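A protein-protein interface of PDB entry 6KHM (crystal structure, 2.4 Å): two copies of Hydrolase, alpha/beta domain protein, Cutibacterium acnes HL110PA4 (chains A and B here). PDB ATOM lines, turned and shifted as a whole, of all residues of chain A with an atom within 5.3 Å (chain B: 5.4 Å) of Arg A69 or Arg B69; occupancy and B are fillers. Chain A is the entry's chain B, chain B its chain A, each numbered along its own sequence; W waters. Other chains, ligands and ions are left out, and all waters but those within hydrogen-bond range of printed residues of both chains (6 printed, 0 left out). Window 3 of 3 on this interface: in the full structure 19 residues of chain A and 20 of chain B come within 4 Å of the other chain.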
ATOM      1  N   GLU A   5      -1.235   8.118   9.311  1.00  0.00           N
ATOM      2  CA  GLU A   5      -0.002   8.622   8.671  1.00  0.00           C
ATOM      3  C   GLU A   5       0.331   9.983   9.281  1.00  0.00           C
ATOM      4  O   GLU A   5      -0.562  10.855   9.294  1.00  0.00           O
ATOM      5  CB  GLU A   5      -0.180   8.682   7.155  1.00  0.00           C
ATOM      6  CG  GLU A   5      -0.092   7.318   6.509  1.00  0.00           C
ATOM      7  CD  GLU A   5      -0.101   7.423   5.004  1.00  0.00           C
ATOM      8  OE1 GLU A   5      -0.148   8.565   4.502  1.00  0.00           O
ATOM      9  OE2 GLU A   5      -0.004   6.367   4.340  1.00  0.00           O
ATOM     10  N   GLN A  18       8.673  10.325   6.890  1.00  0.00           N
ATOM     11  CA  GLN A  18       7.487   9.456   6.764  1.00  0.00           C
ATOM     12  C   GLN A  18       7.359   8.653   8.064  1.00  0.00           C
ATOM     13  O   GLN A  18       8.334   8.016   8.491  1.00  0.00           O
ATOM     14  CB  GLN A  18       7.594   8.646   5.479  1.00  0.00           C
ATOM     15  CG  GLN A  18       7.928   9.500   4.246  1.00  0.00           C
ATOM     16  CD  GLN A  18       6.765  10.327   3.752  1.00  0.00           C
ATOM     17  OE1 GLN A  18       5.818   9.802   3.161  1.00  0.00           O
ATOM     18  NE2 GLN A  18       6.856  11.635   3.940  1.00  0.00           N
ATOM     19  N   TRP A  20       4.237   6.469  10.783  1.00  0.00           N
ATOM     20  CA  TRP A  20       2.949   5.752  10.976  1.00  0.00           C
ATOM     21  C   TRP A  20       2.691   5.534  12.471  1.00  0.00           C
ATOM     22  O   TRP A  20       3.639   5.452  13.248  1.00  0.00           O
ATOM     23  CB  TRP A  20       2.979   4.423  10.218  1.00  0.00           C
ATOM     24  CG  TRP A  20       3.242   4.560   8.753  1.00  0.00           C
ATOM     25  CD1 TRP A  20       2.308   4.709   7.768  1.00  0.00           C
ATOM     26  CD2 TRP A  20       4.531   4.660   8.121  1.00  0.00           C
ATOM     27  NE1 TRP A  20       2.930   4.853   6.553  1.00  0.00           N
ATOM     28  CE2 TRP A  20       4.289   4.791   6.730  1.00  0.00           C
ATOM     29  CE3 TRP A  20       5.854   4.620   8.580  1.00  0.00           C
ATOM     30  CZ2 TRP A  20       5.325   4.918   5.807  1.00  0.00           C
ATOM     31  CZ3 TRP A  20       6.877   4.733   7.661  1.00  0.00           C
ATOM     32  CH2 TRP A  20       6.611   4.917   6.303  1.00  0.00           C
ATOM     33  N   HIS A  41      14.311   0.302   7.239  1.00  0.00           N
ATOM     34  CA  HIS A  41      13.117   1.174   7.363  1.00  0.00           C
ATOM     35  C   HIS A  41      12.133   0.554   8.351  1.00  0.00           C
ATOM     36  O   HIS A  41      12.286  -0.660   8.661  1.00  0.00           O
ATOM     37  CB  HIS A  41      12.443   1.353   5.986  1.00  0.00           C
ATOM     38  CG  HIS A  41      11.962   0.088   5.365  1.00  0.00           C
ATOM     39  ND1 HIS A  41      10.628  -0.224   5.264  1.00  0.00           N
ATOM     40  CD2 HIS A  41      12.631  -0.946   4.828  1.00  0.00           C
ATOM     41  CE1 HIS A  41      10.499  -1.411   4.705  1.00  0.00           C
ATOM     42  NE2 HIS A  41      11.715  -1.888   4.440  1.00  0.00           N
ATOM     43  N   ARG A  43       8.861  -0.179   8.085  1.00  0.00           N
ATOM     44  CA  ARG A  43       7.790  -1.080   7.567  1.00  0.00           C
ATOM     45  C   ARG A  43       8.314  -2.514   7.372  1.00  0.00           C
ATOM     46  O   ARG A  43       7.524  -3.416   7.131  1.00  0.00           O
ATOM     47  CB  ARG A  43       7.167  -0.477   6.311  1.00  0.00           C
ATOM     48  CG  ARG A  43       6.347   0.762   6.651  1.00  0.00           C
ATOM     49  CD  ARG A  43       5.595   1.346   5.505  1.00  0.00           C
ATOM     50  NE  ARG A  43       6.483   1.833   4.464  1.00  0.00           N
ATOM     51  CZ  ARG A  43       6.054   2.265   3.283  1.00  0.00           C
ATOM     52  NH1 ARG A  43       4.762   2.284   3.000  1.00  0.00           N
ATOM     53  NH2 ARG A  43       6.920   2.669   2.385  1.00  0.00           N
ATOM     54  N   ASP A  63      10.524   6.287   9.190  1.00  0.00           N
ATOM     55  CA  ASP A  63      11.736   6.079   8.384  1.00  0.00           C
ATOM     56  C   ASP A  63      12.599   7.304   8.679  1.00  0.00           C
ATOM     57  O   ASP A  63      12.184   8.392   8.356  1.00  0.00           O
ATOM     58  CB  ASP A  63      11.356   5.852   6.928  1.00  0.00           C
ATOM     59  CG  ASP A  63      10.601   4.565   6.704  1.00  0.00           C
ATOM     60  OD1 ASP A  63      10.453   3.827   7.627  1.00  0.00           O
ATOM     61  OD2 ASP A  63      10.180   4.345   5.617  1.00  0.00           O
ATOM     62  N   HIS A  67      16.569   7.532   4.860  1.00  0.00           N
ATOM     63  CA  HIS A  67      16.164   6.098   4.877  1.00  0.00           C
ATOM     64  C   HIS A  67      14.738   5.857   4.389  1.00  0.00           C
ATOM     65  O   HIS A  67      13.871   6.767   4.537  1.00  0.00           O
ATOM     66  CB  HIS A  67      16.346   5.544   6.289  1.00  0.00           C
ATOM     67  CG  HIS A  67      17.780   5.498   6.664  1.00  0.00           C
ATOM     68  ND1 HIS A  67      18.469   6.633   7.004  1.00  0.00           N
ATOM     69  CD2 HIS A  67      18.663   4.484   6.651  1.00  0.00           C
ATOM     70  CE1 HIS A  67      19.732   6.319   7.197  1.00  0.00           C
ATOM     71  NE2 HIS A  67      19.869   5.005   6.992  1.00  0.00           N
ATOM     72  N   GLY A  68      14.509   4.634   3.883  1.00  0.00           N
ATOM     73  CA  GLY A  68      13.166   4.129   3.565  1.00  0.00           C
ATOM     74  C   GLY A  68      12.367   5.168   2.804  1.00  0.00           C
ATOM     75  O   GLY A  68      12.931   5.798   1.883  1.00  0.00           O
ATOM     76  N   ARG A  69      11.088   5.320   3.159  1.00  0.00           N
ATOM     77  CA  ARG A  69      10.103   6.092   2.373  1.00  0.00           C
ATOM     78  C   ARG A  69      10.515   7.558   2.452  1.00  0.00           C
ATOM     79  O   ARG A  69      10.210   8.283   1.513  1.00  0.00           O
ATOM     80  CB  ARG A  69       8.676   5.815   2.863  1.00  0.00           C
ATOM     81  CG  ARG A  69       7.595   6.514   2.043  1.00  0.00           C
ATOM     82  CD  ARG A  69       6.151   6.185   2.420  1.00  0.00           C
ATOM     83  NE  ARG A  69       5.324   6.153   1.230  1.00  0.00           N
ATOM     84  CZ  ARG A  69       4.882   7.229   0.555  1.00  0.00           C
ATOM     85  NH1 ARG A  69       5.140   8.464   0.968  1.00  0.00           N
ATOM     86  NH2 ARG A  69       4.155   7.052  -0.537  1.00  0.00           N
ATOM     87  N   THR A  70      11.228   7.979   3.495  1.00  0.00           N
ATOM     88  CA  THR A  70      11.670   9.401   3.653  1.00  0.00           C
ATOM     89  C   THR A  70      12.669   9.747   2.561  1.00  0.00           C
ATOM     90  O   THR A  70      12.553  10.840   1.956  1.00  0.00           O
ATOM     91  CB  THR A  70      12.329   9.671   5.007  1.00  0.00           C
ATOM     92  OG1 THR A  70      11.307   9.492   5.983  1.00  0.00           O
ATOM     93  CG2 THR A  70      12.942  11.053   5.116  1.00  0.00           C
ATOM     94  N   ALA A  71      13.623   8.842   2.353  1.00  0.00           N
ATOM     95  CA  ALA A  71      14.628   8.913   1.272  1.00  0.00           C
ATOM     96  C   ALA A  71      13.921   8.812  -0.086  1.00  0.00           C
ATOM     97  O   ALA A  71      14.246   9.644  -0.963  1.00  0.00           O
ATOM     98  CB  ALA A  71      15.658   7.833   1.447  1.00  0.00           C
ATOM     99  N   MET A  72      12.958   7.883  -0.217  1.00  0.00           N
ATOM    100  CA  MET A  72      12.289   7.571  -1.491  1.00  0.00           C
ATOM    101  C   MET A  72      11.491   8.811  -1.924  1.00  0.00           C
ATOM    102  O   MET A  72      11.376   9.017  -3.152  1.00  0.00           O
ATOM    103  CB  MET A  72      11.396   6.351  -1.308  1.00  0.00           C
ATOM    104  CG  MET A  72      10.927   5.648  -2.552  1.00  0.00           C
ATOM    105  SD  MET A  72      12.197   4.673  -3.343  1.00  0.00           S
ATOM    106  CE  MET A  72      12.226   3.153  -2.398  1.00  0.00           C
ATOM    107  N   GLN A  73      11.013   9.652  -0.991  1.00  0.00           N
ATOM    108  CA  GLN A  73      10.202  10.857  -1.316  1.00  0.00           C
ATOM    109  C   GLN A  73      11.111  12.057  -1.533  1.00  0.00           C
ATOM    110  O   GLN A  73      10.765  12.864  -2.423  1.00  0.00           O
ATOM    111  CB  GLN A  73       9.182  11.226  -0.241  1.00  0.00           C
ATOM    112  CG  GLN A  73       8.099  10.179  -0.114  1.00  0.00           C
ATOM    113  CD  GLN A  73       7.183  10.058  -1.309  1.00  0.00           C
ATOM    114  OE1 GLN A  73       7.115   9.024  -2.003  1.00  0.00           O
ATOM    115  NE2 GLN A  73       6.392  11.097  -1.502  1.00  0.00           N
ATOM    116  N   SER A  74      12.175  12.194  -0.734  1.00  0.00           N
ATOM    117  CA  SER A  74      13.126  13.346  -0.792  1.00  0.00           C
ATOM    118  C   SER A  74      14.160  13.156  -1.906  1.00  0.00           C
ATOM    119  O   SER A  74      14.650  14.168  -2.374  1.00  0.00           O
ATOM    120  CB  SER A  74      13.840  13.547   0.530  1.00  0.00           C
ATOM    121  OG  SER A  74      14.741  12.472   0.773  1.00  0.00           O
ATOM    122  N   PHE A 208      13.220  -0.556  -0.136  1.00  0.00           N
ATOM    123  CA  PHE A 208      13.149   0.482   0.923  1.00  0.00           C
ATOM    124  C   PHE A 208      14.390   0.413   1.827  1.00  0.00           C
ATOM    125  O   PHE A 208      14.605   1.369   2.588  1.00  0.00           O
ATOM    126  CB  PHE A 208      11.789   0.425   1.631  1.00  0.00           C
ATOM    127  CG  PHE A 208      10.680   1.040   0.817  1.00  0.00           C
ATOM    128  CD1 PHE A 208       9.998   0.294  -0.122  1.00  0.00           C
ATOM    129  CD2 PHE A 208      10.376   2.376   0.926  1.00  0.00           C
ATOM    130  CE1 PHE A 208       9.003   0.856  -0.903  1.00  0.00           C
ATOM    131  CE2 PHE A 208       9.354   2.934   0.164  1.00  0.00           C
ATOM    132  CZ  PHE A 208       8.674   2.174  -0.755  1.00  0.00           C
ATOM    133  N   GLU B   5       5.990  -0.416  -3.282  1.00  0.00           N
ATOM    134  CA  GLU B   5       4.895   0.553  -3.509  1.00  0.00           C
ATOM    135  C   GLU B   5       4.677   0.641  -5.011  1.00  0.00           C
ATOM    136  O   GLU B   5       5.658   0.884  -5.737  1.00  0.00           O
ATOM    137  CB  GLU B   5       5.269   1.929  -2.981  1.00  0.00           C
ATOM    138  CG  GLU B   5       4.850   2.130  -1.566  1.00  0.00           C
ATOM    139  CD  GLU B   5       5.194   3.502  -1.041  1.00  0.00           C
ATOM    140  OE1 GLU B   5       5.390   4.424  -1.865  1.00  0.00           O
ATOM    141  OE2 GLU B   5       5.264   3.635   0.198  1.00  0.00           O
ATOM    142  N   GLN B  18      -3.420   3.667  -4.803  1.00  0.00           N
ATOM    143  CA  GLN B  18      -2.364   3.416  -3.799  1.00  0.00           C
ATOM    144  C   GLN B  18      -2.311   1.910  -3.518  1.00  0.00           C
ATOM    145  O   GLN B  18      -3.274   1.318  -3.003  1.00  0.00           O
ATOM    146  CB  GLN B  18      -2.645   4.274  -2.569  1.00  0.00           C
ATOM    147  CG  GLN B  18      -2.773   5.754  -2.911  1.00  0.00           C
ATOM    148  CD  GLN B  18      -1.503   6.340  -3.473  1.00  0.00           C
ATOM    149  OE1 GLN B  18      -0.451   6.296  -2.827  1.00  0.00           O
ATOM    150  NE2 GLN B  18      -1.597   6.897  -4.662  1.00  0.00           N
ATOM    151  N   TRP B  20       0.320  -1.733  -2.687  1.00  0.00           N
ATOM    152  CA  TRP B  20       1.537  -2.325  -2.096  1.00  0.00           C
ATOM    153  C   TRP B  20       1.617  -3.788  -2.503  1.00  0.00           C
ATOM    154  O   TRP B  20       0.564  -4.429  -2.640  1.00  0.00           O
ATOM    155  CB  TRP B  20       1.501  -2.176  -0.569  1.00  0.00           C
ATOM    156  CG  TRP B  20       1.325  -0.762  -0.095  1.00  0.00           C
ATOM    157  CD1 TRP B  20       2.304   0.120   0.260  1.00  0.00           C
ATOM    158  CD2 TRP B  20       0.091  -0.035   0.021  1.00  0.00           C
ATOM    159  NE1 TRP B  20       1.764   1.329   0.629  1.00  0.00           N
ATOM    160  CE2 TRP B  20       0.404   1.252   0.521  1.00  0.00           C
ATOM    161  CE3 TRP B  20      -1.255  -0.347  -0.222  1.00  0.00           C
ATOM    162  CZ2 TRP B  20      -0.576   2.227   0.748  1.00  0.00           C
ATOM    163  CZ3 TRP B  20      -2.226   0.603   0.043  1.00  0.00           C
ATOM    164  CH2 TRP B  20      -1.888   1.878   0.511  1.00  0.00           C
ATOM    165  N   HIS B  41     -10.042  -0.197   4.084  1.00  0.00           N
ATOM    166  CA  HIS B  41      -8.783  -0.087   3.298  1.00  0.00           C
ATOM    167  C   HIS B  41      -7.935  -1.356   3.440  1.00  0.00           C
ATOM    168  O   HIS B  41      -8.190  -2.109   4.327  1.00  0.00           O
ATOM    169  CB  HIS B  41      -7.987   1.159   3.729  1.00  0.00           C
ATOM    170  CG  HIS B  41      -7.586   1.150   5.166  1.00  0.00           C
ATOM    171  ND1 HIS B  41      -6.272   1.050   5.566  1.00  0.00           N
ATOM    172  CD2 HIS B  41      -8.328   1.257   6.292  1.00  0.00           C
ATOM    173  CE1 HIS B  41      -6.225   1.126   6.871  1.00  0.00           C
ATOM    174  NE2 HIS B  41      -7.470   1.258   7.338  1.00  0.00           N
ATOM    175  N   ARG B  43      -4.646  -1.775   4.207  1.00  0.00           N
ATOM    176  CA  ARG B  43      -3.691  -1.824   5.354  1.00  0.00           C
ATOM    177  C   ARG B  43      -4.431  -2.151   6.664  1.00  0.00           C
ATOM    178  O   ARG B  43      -3.778  -2.212   7.684  1.00  0.00           O
ATOM    179  CB  ARG B  43      -2.854  -0.546   5.408  1.00  0.00           C
ATOM    180  CG  ARG B  43      -1.830  -0.473   4.284  1.00  0.00           C
ATOM    181  CD  ARG B  43      -1.009   0.806   4.243  1.00  0.00           C
ATOM    182  NE  ARG B  43      -1.819   2.010   4.181  1.00  0.00           N
ATOM    183  CZ  ARG B  43      -1.346   3.248   4.344  1.00  0.00           C
ATOM    184  NH1 ARG B  43      -0.055   3.460   4.584  1.00  0.00           N
ATOM    185  NH2 ARG B  43      -2.191   4.276   4.301  1.00  0.00           N
ATOM    186  N   ASP B  63      -5.689   0.260  -2.277  1.00  0.00           N
ATOM    187  CA  ASP B  63      -6.858   0.938  -1.699  1.00  0.00           C
ATOM    188  C   ASP B  63      -7.649   1.307  -2.938  1.00  0.00           C
ATOM    189  O   ASP B  63      -7.130   2.024  -3.743  1.00  0.00           O
ATOM    190  CB  ASP B  63      -6.446   2.122  -0.840  1.00  0.00           C
ATOM    191  CG  ASP B  63      -5.908   1.694   0.499  1.00  0.00           C
ATOM    192  OD1 ASP B  63      -5.946   0.543   0.771  1.00  0.00           O
ATOM    193  OD2 ASP B  63      -5.470   2.534   1.222  1.00  0.00           O
ATOM    194  N   HIS B  67     -11.345   5.205  -1.683  1.00  0.00           N
ATOM    195  CA  HIS B  67     -11.072   4.530  -0.389  1.00  0.00           C
ATOM    196  C   HIS B  67      -9.611   4.661   0.043  1.00  0.00           C
ATOM    197  O   HIS B  67      -8.740   4.875  -0.792  1.00  0.00           O
ATOM    198  CB  HIS B  67     -11.449   3.044  -0.478  1.00  0.00           C
ATOM    199  CG  HIS B  67     -12.913   2.774  -0.581  1.00  0.00           C
ATOM    200  ND1 HIS B  67     -13.613   2.941  -1.728  1.00  0.00           N
ATOM    201  CD2 HIS B  67     -13.799   2.346   0.321  1.00  0.00           C
ATOM    202  CE1 HIS B  67     -14.857   2.672  -1.526  1.00  0.00           C
ATOM    203  NE2 HIS B  67     -14.986   2.289  -0.294  1.00  0.00           N
ATOM    204  N   GLY B  68      -9.400   4.494   1.340  1.00  0.00           N
ATOM    205  CA  GLY B  68      -8.096   4.540   2.008  1.00  0.00           C
ATOM    206  C   GLY B  68      -7.204   5.687   1.591  1.00  0.00           C
ATOM    207  O   GLY B  68      -7.667   6.813   1.510  1.00  0.00           O
ATOM    208  N   ARG B  69      -5.956   5.347   1.311  1.00  0.00           N
ATOM    209  CA  ARG B  69      -4.855   6.288   0.985  1.00  0.00           C
ATOM    210  C   ARG B  69      -5.158   6.923  -0.375  1.00  0.00           C
ATOM    211  O   ARG B  69      -4.787   8.099  -0.549  1.00  0.00           O
ATOM    212  CB  ARG B  69      -3.495   5.574   1.015  1.00  0.00           C
ATOM    213  CG  ARG B  69      -2.313   6.540   1.050  1.00  0.00           C
ATOM    214  CD  ARG B  69      -0.968   5.869   1.289  1.00  0.00           C
ATOM    215  NE  ARG B  69      -0.049   6.896   1.731  1.00  0.00           N
ATOM    216  CZ  ARG B  69       0.558   7.776   0.933  1.00  0.00           C
ATOM    217  NH1 ARG B  69       0.355   7.754  -0.372  1.00  0.00           N
ATOM    218  NH2 ARG B  69       1.372   8.677   1.445  1.00  0.00           N
ATOM    219  N   THR B  70      -5.830   6.185  -1.269  1.00  0.00           N
ATOM    220  CA  THR B  70      -6.233   6.654  -2.625  1.00  0.00           C
ATOM    221  C   THR B  70      -7.219   7.818  -2.497  1.00  0.00           C
ATOM    222  O   THR B  70      -7.078   8.787  -3.249  1.00  0.00           O
ATOM    223  CB  THR B  70      -6.868   5.527  -3.451  1.00  0.00           C
ATOM    224  OG1 THR B  70      -5.872   4.542  -3.731  1.00  0.00           O
ATOM    225  CG2 THR B  70      -7.521   6.015  -4.733  1.00  0.00           C
ATOM    226  N   ALA B  71      -8.193   7.718  -1.596  1.00  0.00           N
ATOM    227  CA  ALA B  71      -9.121   8.826  -1.261  1.00  0.00           C
ATOM    228  C   ALA B  71      -8.340   9.962  -0.572  1.00  0.00           C
ATOM    229  O   ALA B  71      -8.605  11.161  -0.826  1.00  0.00           O
ATOM    230  CB  ALA B  71     -10.252   8.319  -0.389  1.00  0.00           C
ATOM    231  N   MET B  72      -7.420   9.592   0.311  1.00  0.00           N
ATOM    232  CA  MET B  72      -6.644  10.526   1.164  1.00  0.00           C
ATOM    233  C   MET B  72      -5.769  11.401   0.230  1.00  0.00           C
ATOM    234  O   MET B  72      -5.695  12.608   0.481  1.00  0.00           O
ATOM    235  CB  MET B  72      -5.858   9.682   2.184  1.00  0.00           C
ATOM    236  CG  MET B  72      -5.421  10.386   3.463  1.00  0.00           C
ATOM    237  SD  MET B  72      -6.760  11.014   4.520  1.00  0.00           S
ATOM    238  CE  MET B  72      -7.032   9.631   5.633  1.00  0.00           C
ATOM    239  N   GLN B  73      -5.294  10.881  -0.912  1.00  0.00           N
ATOM    240  CA  GLN B  73      -4.405  11.608  -1.866  1.00  0.00           C
ATOM    241  C   GLN B  73      -5.187  12.316  -2.997  1.00  0.00           C
ATOM    242  O   GLN B  73      -4.650  13.317  -3.586  1.00  0.00           O
ATOM    243  CB  GLN B  73      -3.408  10.628  -2.490  1.00  0.00           C
ATOM    244  CG  GLN B  73      -2.459   9.983  -1.486  1.00  0.00           C
ATOM    245  CD  GLN B  73      -1.471  10.977  -0.917  1.00  0.00           C
ATOM    246  OE1 GLN B  73      -1.408  11.191   0.289  1.00  0.00           O
ATOM    247  NE2 GLN B  73      -0.717  11.613  -1.793  1.00  0.00           N
ATOM    248  N   SER B  74      -6.337  11.773  -3.400  1.00  0.00           N
ATOM    249  CA  SER B  74      -7.229  12.362  -4.427  1.00  0.00           C
ATOM    250  C   SER B  74      -8.113  13.406  -3.748  1.00  0.00           C
ATOM    251  O   SER B  74      -8.516  14.341  -4.426  1.00  0.00           O
ATOM    252  CB  SER B  74      -8.083  11.313  -5.087  1.00  0.00           C
ATOM    253  OG  SER B  74      -9.104  10.869  -4.183  1.00  0.00           O
ATOM    254  N   PHE B 208      -8.389   5.942   7.972  1.00  0.00           N
ATOM    255  CA  PHE B 208      -8.262   5.432   6.595  1.00  0.00           C
ATOM    256  C   PHE B 208      -9.535   4.688   6.185  1.00  0.00           C
ATOM    257  O   PHE B 208      -9.632   4.309   5.041  1.00  0.00           O
ATOM    258  CB  PHE B 208      -6.930   4.703   6.412  1.00  0.00           C
ATOM    259  CG  PHE B 208      -5.751   5.626   6.320  1.00  0.00           C
ATOM    260  CD1 PHE B 208      -5.084   6.039   7.444  1.00  0.00           C
ATOM    261  CD2 PHE B 208      -5.339   6.114   5.102  1.00  0.00           C
ATOM    262  CE1 PHE B 208      -4.012   6.899   7.343  1.00  0.00           C
ATOM    263  CE2 PHE B 208      -4.262   6.969   5.005  1.00  0.00           C
ATOM    264  CZ  PHE B 208      -3.606   7.368   6.128  1.00  0.00           C
HETATM  265  O   HOH W   1       7.696   6.407  -1.677  1.00  0.00           O
HETATM  266  O   HOH W   2      -2.214   9.708   2.961  1.00  0.00           O
HETATM  267  O   HOH W   3       2.451   4.164   1.161  1.00  0.00           O
HETATM  268  O   HOH W   4       1.801   4.668  -1.254  1.00  0.00           O
HETATM  269  O   HOH W   5       2.390   1.650   4.505  1.00  0.00           O
HETATM  270  O   HOH W   6       3.253   8.029   4.294  1.00  0.00           O
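The side-chain carboxylate of Glu B5 is in salt-bridge range of the guanidinium group of Arg A43. OE2 of Glu B5 lies within salt-bridge range of NE of Arg A69. The guanidinium group of Arg B43 lies within salt-bridge range of the side-chain carboxylate of Glu A5, 2.9 Å away. The guanidinium group of Arg B69 lies within salt-bridge range of the side-chain carboxylate of Glu A5 (2.7 Å).
The side-chain amide oxygen (OE1) of Gln B18 lies within hydrogen-bond range of the guanidinium group (NH1) of Arg B69 (3.0 Å). The side-chain carboxylate (OD2) of Asp B63 lies within hydrogen-bond range of the backbone NH (N) of Arg B69. The side-chain amide oxygen of Gln A18 sits at hydrogen-bond distance from the guanidinium group of Arg A69, 2.7 Å away. ND1 of His A41 lies within hydrogen-bond range of N of Arg A43 (3.3 Å). The backbone NH (N) of Arg A69 lies within hydrogen-bond range of the side-chain carboxylate (OD2) of Asp A63 (2.8 Å).
CG of Glu A5 touches CZ of Phe B208, at 3.5 Å. Arg B43 touches Trp A20 (NH1 to NE1, 3.8 Å). Trp B20 touches Arg A43 (NE1 to NH1, 3.9 Å). NH2 of Arg A69 touches NH2 of Arg B69, at 3.8 Å. Phe A208 touches Glu B5 (CZ to CD, 3.7 Å).
Printed residues of chain B within 4 Å of Arg A43: Glu B5 and Trp B20. Asp A63 touches none of the printed residues of chain B. Of chain B, only Glu B5 (2.7 Å) and Arg B69 (3.8 Å) come within 4 Å of Arg A69. Of the printed residues of chain B, Phe A208 touches Glu B5 (3.7 Å). Printed residues of chain A within 4 Å of Glu B5: Arg A43 (2.9 Å), Arg A69 (2.7 Å) and Phe A208 (3.7 Å). His B67 touches none of the printed residues of chain A. Arg B69 touches two residues of chain A. Of the printed residues of chain A, Phe B208 touches Glu A5. The nearest residue of chain B that does not touch Arg A69 is Gln B18 (5.2 Å). The nearest residue of chain A that does not touch Arg B69 is Gln A18 (4.9 Å).
Of the 15 printed residues of chain B, 5 touch a printed residue of chain A. Hydrophobic or aromatic side chains of chain B that line the printed part of chain A: Trp B20 and Phe B208. Of the 15 printed residues of chain A, 5 touch a printed residue of chain B.
Glu A5 touches Arg B43, and with the chains exchanged Arg A43 touches Glu B5. Glu A5 touches Phe B208, and with the chains exchanged Phe A208 touches Glu B5. Trp A20 touches Arg B43, and with the chains exchanged Arg A43 touches Trp B20. Arg B69 touches its own counterpart, Arg A69. Positions printed for both chains: 5, 18, 20, 41, 43, 63, 67, 68, 69, 70, 71, 72, 73, 74 and 208.
Water W1 bridges OE1 of Gln A73 (2.7 Å) and OE1 of Glu B5 (3.0 Å). Water W2 lies within hydrogen-bond range of OE1 of Glu A5 and OE1 of Gln B73. Water W5 bridges NH1 of Arg A43 (2.9 Å) and NH1 of Arg B43 (3.0 Å). Water W3 lies within hydrogen-bond range of NE1 of Trp B20 (3.0 Å), OE2 of Glu B5 (3.0 Å) and NE of Arg A69 (3.5 Å). Water W4 bridges OE1 of Gln B18 (3.2 Å) and NH2 of Arg A69 (3.4 Å). Water W6 lies within hydrogen-bond range of the side-chain amide oxygen (OE1) of Gln A18, the side-chain carboxylate (OE1) of Glu A5 and the guanidinium group (NH2) of Arg B69.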
